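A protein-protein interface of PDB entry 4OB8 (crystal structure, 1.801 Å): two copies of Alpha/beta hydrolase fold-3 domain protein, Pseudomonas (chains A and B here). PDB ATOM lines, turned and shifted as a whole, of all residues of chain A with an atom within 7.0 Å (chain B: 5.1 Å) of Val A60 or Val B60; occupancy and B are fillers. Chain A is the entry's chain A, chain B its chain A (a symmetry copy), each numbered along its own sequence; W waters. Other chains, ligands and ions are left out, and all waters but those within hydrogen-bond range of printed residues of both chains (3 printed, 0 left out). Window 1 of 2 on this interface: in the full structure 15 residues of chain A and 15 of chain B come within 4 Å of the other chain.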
ATOM      1  N   GLN A  55       1.356 -33.580  14.440  1.00  0.00           N
ATOM      2  CA  GLN A  55       0.254 -32.824  13.842  1.00  0.00           C
ATOM      3  C   GLN A  55       0.009 -31.518  14.594  1.00  0.00           C
ATOM      4  O   GLN A  55      -0.388 -30.513  14.007  1.00  0.00           O
ATOM      5  CB  GLN A  55      -1.032 -33.666  13.786  1.00  0.00           C
ATOM      6  CG  GLN A  55      -0.967 -34.856  12.823  1.00  0.00           C
ATOM      7  CD  GLN A  55      -0.808 -34.415  11.375  1.00  0.00           C
ATOM      8  OE1 GLN A  55       0.279 -34.024  10.951  1.00  0.00           O
ATOM      9  NE2 GLN A  55      -1.900 -34.461  10.616  1.00  0.00           N
ATOM     10  N   VAL A  58       2.347 -27.713  14.177  1.00  0.00           N
ATOM     11  CA  VAL A  58       2.283 -26.904  12.972  1.00  0.00           C
ATOM     12  C   VAL A  58       1.048 -26.020  13.007  1.00  0.00           C
ATOM     13  O   VAL A  58      -0.058 -26.517  13.192  1.00  0.00           O
ATOM     14  CB  VAL A  58       2.121 -27.823  11.734  1.00  0.00           C
ATOM     15  CG1 VAL A  58       2.280 -27.032  10.476  1.00  0.00           C
ATOM     16  CG2 VAL A  58       3.126 -28.954  11.771  1.00  0.00           C
ATOM     17  N   LYS A  59       1.216 -24.713  12.821  1.00  0.00           N
ATOM     18  CA  LYS A  59       0.041 -23.854  12.677  1.00  0.00           C
ATOM     19  C   LYS A  59      -0.682 -24.182  11.365  1.00  0.00           C
ATOM     20  O   LYS A  59      -0.065 -24.144  10.298  1.00  0.00           O
ATOM     21  CB  LYS A  59       0.454 -22.384  12.687  1.00  0.00           C
ATOM     22  CG  LYS A  59      -0.671 -21.424  12.353  1.00  0.00           C
ATOM     23  CD  LYS A  59      -0.224 -19.983  12.537  1.00  0.00           C
ATOM     24  CE  LYS A  59       0.892 -19.632  11.580  1.00  0.00           C
ATOM     25  NZ  LYS A  59       0.467 -18.559  10.635  1.00  0.00           N
ATOM     26  N   VAL A  60      -1.973 -24.514  11.443  1.00  0.00           N
ATOM     27  CA  VAL A  60      -2.765 -24.819  10.243  1.00  0.00           C
ATOM     28  C   VAL A  60      -4.121 -24.121  10.250  1.00  0.00           C
ATOM     29  O   VAL A  60      -4.688 -23.831  11.315  1.00  0.00           O
ATOM     30  CB  VAL A  60      -2.998 -26.342  10.043  1.00  0.00           C
ATOM     31  CG1 VAL A  60      -1.693 -27.058   9.743  1.00  0.00           C
ATOM     32  CG2 VAL A  60      -3.702 -26.957  11.255  1.00  0.00           C
ATOM     33  N   ASP A  61      -4.644 -23.867   9.052  1.00  0.00           N
ATOM     34  CA  ASP A  61      -5.958 -23.233   8.912  1.00  0.00           C
ATOM     35  C   ASP A  61      -7.062 -24.272   9.092  1.00  0.00           C
ATOM     36  O   ASP A  61      -7.163 -25.205   8.296  1.00  0.00           O
ATOM     37  CB  ASP A  61      -6.064 -22.601   7.521  1.00  0.00           C
ATOM     38  CG  ASP A  61      -7.292 -21.716   7.351  1.00  0.00           C
ATOM     39  OD1 ASP A  61      -8.164 -21.690   8.238  1.00  0.00           O
ATOM     40  OD2 ASP A  61      -7.385 -21.041   6.301  1.00  0.00           O
ATOM     41  N   LEU A  62      -7.879 -24.118  10.135  1.00  0.00           N
ATOM     42  CA  LEU A  62      -9.023 -25.012  10.360  1.00  0.00           C
ATOM     43  C   LEU A  62     -10.355 -24.278  10.250  1.00  0.00           C
ATOM     44  O   LEU A  62     -11.386 -24.797  10.677  1.00  0.00           O
ATOM     45  CB  LEU A  62      -8.928 -25.693  11.736  1.00  0.00           C
ATOM     46  CG  LEU A  62      -7.729 -26.619  11.955  1.00  0.00           C
ATOM     47  CD1 LEU A  62      -7.713 -27.194  13.360  1.00  0.00           C
ATOM     48  CD2 LEU A  62      -7.751 -27.744  10.932  1.00  0.00           C
ATOM     49  N   SER A  63     -10.337 -23.080   9.670  1.00  0.00           N
ATOM     50  CA  SER A  63     -11.540 -22.244   9.590  1.00  0.00           C
ATOM     51  C   SER A  63     -12.554 -22.772   8.579  1.00  0.00           C
ATOM     52  O   SER A  63     -12.242 -23.636   7.760  1.00  0.00           O
ATOM     53  CB  SER A  63     -11.167 -20.805   9.224  1.00  0.00           C
ATOM     54  OG  SER A  63     -10.654 -20.732   7.903  1.00  0.00           O
ATOM     55  N   GLN A 113      -7.941 -33.759  11.470  1.00  0.00           N
ATOM     56  CA  GLN A 113      -8.908 -32.679  11.310  1.00  0.00           C
ATOM     57  C   GLN A 113      -8.574 -31.716  10.178  1.00  0.00           C
ATOM     58  O   GLN A 113      -9.472 -31.244   9.484  1.00  0.00           O
ATOM     59  CB  GLN A 113      -9.106 -31.906  12.618  1.00  0.00           C
ATOM     60  CG  GLN A 113     -10.248 -30.910  12.529  1.00  0.00           C
ATOM     61  CD  GLN A 113     -10.593 -30.300  13.859  1.00  0.00           C
ATOM     62  OE1 GLN A 113      -9.780 -30.290  14.792  1.00  0.00           O
ATOM     63  NE2 GLN A 113     -11.809 -29.793  13.965  1.00  0.00           N
ATOM     64  N   ARG A 114      -7.293 -31.422   9.974  1.00  0.00           N
ATOM     65  CA  ARG A 114      -6.940 -30.487   8.910  1.00  0.00           C
ATOM     66  C   ARG A 114      -7.264 -31.060   7.528  1.00  0.00           C
ATOM     67  O   ARG A 114      -7.813 -30.359   6.679  1.00  0.00           O
ATOM     68  CB  ARG A 114      -5.469 -30.066   8.995  1.00  0.00           C
ATOM     69  CG  ARG A 114      -5.172 -28.768   8.227  1.00  0.00           C
ATOM     70  CD  ARG A 114      -3.986 -28.932   7.275  1.00  0.00           C
ATOM     71  NE  ARG A 114      -4.373 -29.590   6.019  1.00  0.00           N
ATOM     72  CZ  ARG A 114      -3.921 -30.776   5.623  1.00  0.00           C
ATOM     73  NH1 ARG A 114      -4.320 -31.284   4.462  1.00  0.00           N
ATOM     74  NH2 ARG A 114      -3.069 -31.459   6.390  1.00  0.00           N
ATOM     75  N   LEU A 306      -0.169 -35.197   6.627  1.00  0.00           N
ATOM     76  CA  LEU A 306       0.879 -34.630   7.476  1.00  0.00           C
ATOM     77  C   LEU A 306       0.877 -33.099   7.489  1.00  0.00           C
ATOM     78  O   LEU A 306       1.107 -32.451   6.470  1.00  0.00           O
ATOM     79  CB  LEU A 306       2.253 -35.155   7.044  1.00  0.00           C
ATOM     80  CG  LEU A 306       2.381 -36.680   6.934  1.00  0.00           C
ATOM     81  CD1 LEU A 306       3.783 -37.065   6.496  1.00  0.00           C
ATOM     82  CD2 LEU A 306       2.021 -37.382   8.247  1.00  0.00           C
ATOM     83  N   ASN A 307       0.615 -32.515   8.650  1.00  0.00           N
ATOM     84  CA  ASN A 307       0.535 -31.062   8.727  1.00  0.00           C
ATOM     85  C   ASN A 307       1.802 -30.306   8.306  1.00  0.00           C
ATOM     86  O   ASN A 307       1.692 -29.223   7.738  1.00  0.00           O
ATOM     87  CB  ASN A 307       0.009 -30.610  10.094  1.00  0.00           C
ATOM     88  CG  ASN A 307      -1.459 -30.912  10.259  1.00  0.00           C
ATOM     89  OD1 ASN A 307      -2.153 -31.148   9.265  1.00  0.00           O
ATOM     90  ND2 ASN A 307      -1.955 -30.901  11.501  1.00  0.00           N
ATOM     91  N   PRO A 308       3.000 -30.867   8.567  1.00  0.00           N
ATOM     92  CA  PRO A 308       4.189 -30.167   8.066  1.00  0.00           C
ATOM     93  C   PRO A 308       4.252 -30.053   6.542  1.00  0.00           C
ATOM     94  O   PRO A 308       5.052 -29.255   6.045  1.00  0.00           O
ATOM     95  CB  PRO A 308       5.345 -31.045   8.559  1.00  0.00           C
ATOM     96  CG  PRO A 308       4.828 -31.662   9.811  1.00  0.00           C
ATOM     97  CD  PRO A 308       3.368 -31.925   9.534  1.00  0.00           C
ATOM     98  N   SER A 310       1.352 -29.515   4.692  1.00  0.00           N
ATOM     99  CA  SER A 310       0.025 -29.043   4.280  1.00  0.00           C
ATOM    100  C   SER A 310       0.036 -27.798   3.389  1.00  0.00           C
ATOM    101  O   SER A 310      -0.968 -27.506   2.724  1.00  0.00           O
ATOM    102  CB  SER A 310      -0.864 -28.799   5.503  1.00  0.00           C
ATOM    103  OG  SER A 310      -0.350 -27.754   6.308  1.00  0.00           O
ATOM    104  N   GLN A 311       1.158 -27.078   3.365  1.00  0.00           N
ATOM    105  CA  GLN A 311       1.289 -25.885   2.522  1.00  0.00           C
ATOM    106  C   GLN A 311       2.166 -26.120   1.288  1.00  0.00           C
ATOM    107  O   GLN A 311       2.422 -25.194   0.518  1.00  0.00           O
ATOM    108  CB  GLN A 311       1.840 -24.700   3.324  1.00  0.00           C
ATOM    109  CG  GLN A 311       0.894 -24.159   4.389  1.00  0.00           C
ATOM    110  CD  GLN A 311      -0.451 -23.738   3.825  1.00  0.00           C
ATOM    111  OE1 GLN A 311      -1.498 -24.190   4.287  1.00  0.00           O
ATOM    112  NE2 GLN A 311      -0.426 -22.873   2.815  1.00  0.00           N
ATOM    113  N   VAL B  58     -12.863 -17.122  10.551  1.00  0.00           N
ATOM    114  CA  VAL B  58     -11.564 -16.502  10.750  1.00  0.00           C
ATOM    115  C   VAL B  58     -10.489 -17.571  10.846  1.00  0.00           C
ATOM    116  O   VAL B  58     -10.603 -18.486  11.654  1.00  0.00           O
ATOM    117  CB  VAL B  58     -11.546 -15.750  12.106  1.00  0.00           C
ATOM    118  CG1 VAL B  58     -10.307 -14.923  12.225  1.00  0.00           C
ATOM    119  CG2 VAL B  58     -12.773 -14.877  12.250  1.00  0.00           C
ATOM    120  N   LYS B  59      -9.437 -17.466  10.038  1.00  0.00           N
ATOM    121  CA  LYS B  59      -8.304 -18.374  10.216  1.00  0.00           C
ATOM    122  C   LYS B  59      -7.604 -18.072  11.546  1.00  0.00           C
ATOM    123  O   LYS B  59      -7.202 -16.931  11.784  1.00  0.00           O
ATOM    124  CB  LYS B  59      -7.314 -18.220   9.064  1.00  0.00           C
ATOM    125  CG  LYS B  59      -6.018 -18.982   9.258  1.00  0.00           C
ATOM    126  CD  LYS B  59      -5.156 -18.908   8.008  1.00  0.00           C
ATOM    127  CE  LYS B  59      -4.738 -17.485   7.716  1.00  0.00           C
ATOM    128  NZ  LYS B  59      -3.258 -17.336   7.801  1.00  0.00           N
ATOM    129  N   VAL B  60      -7.471 -19.081  12.412  1.00  0.00           N
ATOM    130  CA  VAL B  60      -6.791 -18.905  13.703  1.00  0.00           C
ATOM    131  C   VAL B  60      -5.804 -20.029  13.997  1.00  0.00           C
ATOM    132  O   VAL B  60      -5.968 -21.167  13.528  1.00  0.00           O
ATOM    133  CB  VAL B  60      -7.779 -18.794  14.898  1.00  0.00           C
ATOM    134  CG1 VAL B  60      -8.603 -17.523  14.806  1.00  0.00           C
ATOM    135  CG2 VAL B  60      -8.675 -20.031  14.989  1.00  0.00           C
ATOM    136  N   ASP B  61      -4.783 -19.708  14.789  1.00  0.00           N
ATOM    137  CA  ASP B  61      -3.780 -20.701  15.183  1.00  0.00           C
ATOM    138  C   ASP B  61      -4.310 -21.553  16.333  1.00  0.00           C
ATOM    139  O   ASP B  61      -4.563 -21.031  17.418  1.00  0.00           O
ATOM    140  CB  ASP B  61      -2.502 -19.978  15.620  1.00  0.00           C
ATOM    141  CG  ASP B  61      -1.319 -20.913  15.825  1.00  0.00           C
ATOM    142  OD1 ASP B  61      -1.489 -22.145  15.787  1.00  0.00           O
ATOM    143  OD2 ASP B  61      -0.198 -20.399  16.038  1.00  0.00           O
ATOM    144  N   LEU B  62      -4.484 -22.854  16.098  1.00  0.00           N
ATOM    145  CA  LEU B  62      -4.914 -23.781  17.154  1.00  0.00           C
ATOM    146  C   LEU B  62      -3.843 -24.818  17.478  1.00  0.00           C
ATOM    147  O   LEU B  62      -4.131 -25.824  18.124  1.00  0.00           O
ATOM    148  CB  LEU B  62      -6.217 -24.498  16.762  1.00  0.00           C
ATOM    149  CG  LEU B  62      -7.450 -23.612  16.571  1.00  0.00           C
ATOM    150  CD1 LEU B  62      -8.661 -24.419  16.139  1.00  0.00           C
ATOM    151  CD2 LEU B  62      -7.754 -22.864  17.861  1.00  0.00           C
ATOM    152  N   ARG B 114     -10.223 -21.512  20.456  1.00  0.00           N
ATOM    153  CA  ARG B 114      -9.042 -20.674  20.270  1.00  0.00           C
ATOM    154  C   ARG B 114      -8.627 -19.994  21.578  1.00  0.00           C
ATOM    155  O   ARG B 114      -7.442 -19.960  21.909  1.00  0.00           O
ATOM    156  CB  ARG B 114      -9.255 -19.639  19.161  1.00  0.00           C
ATOM    157  CG  ARG B 114      -7.937 -19.068  18.613  1.00  0.00           C
ATOM    158  CD  ARG B 114      -7.943 -17.538  18.605  1.00  0.00           C
ATOM    159  NE  ARG B 114      -7.639 -16.976  19.928  1.00  0.00           N
ATOM    160  CZ  ARG B 114      -8.490 -16.252  20.648  1.00  0.00           C
ATOM    161  NH1 ARG B 114      -8.119 -15.775  21.832  1.00  0.00           N
ATOM    162  NH2 ARG B 114      -9.716 -16.003  20.188  1.00  0.00           N
ATOM    163  N   ASN B 307     -12.987 -14.468  17.590  1.00  0.00           N
ATOM    164  CA  ASN B 307     -11.882 -14.734  16.678  1.00  0.00           C
ATOM    165  C   ASN B 307     -11.494 -13.576  15.751  1.00  0.00           C
ATOM    166  O   ASN B 307     -10.314 -13.421  15.448  1.00  0.00           O
ATOM    167  CB  ASN B 307     -12.100 -16.047  15.917  1.00  0.00           C
ATOM    168  CG  ASN B 307     -11.932 -17.250  16.811  1.00  0.00           C
ATOM    169  OD1 ASN B 307     -11.343 -17.135  17.890  1.00  0.00           O
ATOM    170  ND2 ASN B 307     -12.432 -18.413  16.380  1.00  0.00           N
ATOM    171  N   SER B 310      -8.773 -11.739  17.516  1.00  0.00           N
ATOM    172  CA  SER B 310      -7.743 -12.555  18.169  1.00  0.00           C
ATOM    173  C   SER B 310      -6.303 -12.120  17.879  1.00  0.00           C
ATOM    174  O   SER B 310      -5.383 -12.509  18.611  1.00  0.00           O
ATOM    175  CB  SER B 310      -7.921 -14.033  17.816  1.00  0.00           C
ATOM    176  OG  SER B 310      -7.724 -14.255  16.432  1.00  0.00           O
HETATM  177  O   HOH W   1      -3.625 -20.528  11.034  1.00  0.00           O
HETATM  178  O   HOH W   2      -8.190 -22.057  12.110  1.00  0.00           O
HETATM  179  O   HOH W   3      -3.863 -24.556  13.871  1.00  0.00           O
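The side-chain carboxylate of Asp A61 sits at hydrogen-bond distance from the side-chain hydroxyl of Ser A63.
Among the printed residues, merely in contact across the chains: Ser A63 with Val B58, Lys A59 with Asp B61, Asp A61 with Lys B59, Val A60 with Val B60 and Ser A63 with Lys B59.
Val A60 touches just one residue of chain B: Val B60 (3.7 Å).
Val B60 touches one residue of chain A.
Printed residues of chain B within 4 Å of Asp A61: Lys B59 (3.5 Å).
Of the printed residues of chain A, Val B58 touches Ser A63 (3.4 Å).
Of the printed residues of chain B, Lys A59 touches Asp B61.
Of the printed residues of chain A, Asp B61 touches Lys A59 (3.5 Å).
The nearest residue of chain B that does not touch Val A60 is Leu B62 (4.9 Å).
The nearest residue of chain A that does not touch Val B60 is Leu A62 (4.9 Å).
The nearest printed residue of chain B that does not touch Asp A61 is Val B60 (5.0 Å).
Printed residues of chain B that touch a printed residue of chain A: Val B58, Lys B59, Val B60 and Asp B61.
Among the printed residues, 5 pairs touch across the chains.
Among the printed residues, no Asp or Glu carboxylate lies within 4 Å of a Lys or Arg side-chain nitrogen of the other chain.
Lys A59 touches Asp B61, and with the chains exchanged Asp A61 touches Lys B59.
Val B60 touches its own counterpart, Val A60.
8 positions are printed for both chains.
Water W2 lies within hydrogen-bond range of O of Val B60, N of Leu A62 and N of Ser A63.
Water W3 bridges O of Val A60 (2.8 Å) and N of Leu B62 (2.9 Å).
Water W1 lies within hydrogen-bond range of O of Val A60 (3.5 Å) and O of Val B60 (3.5 Å).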
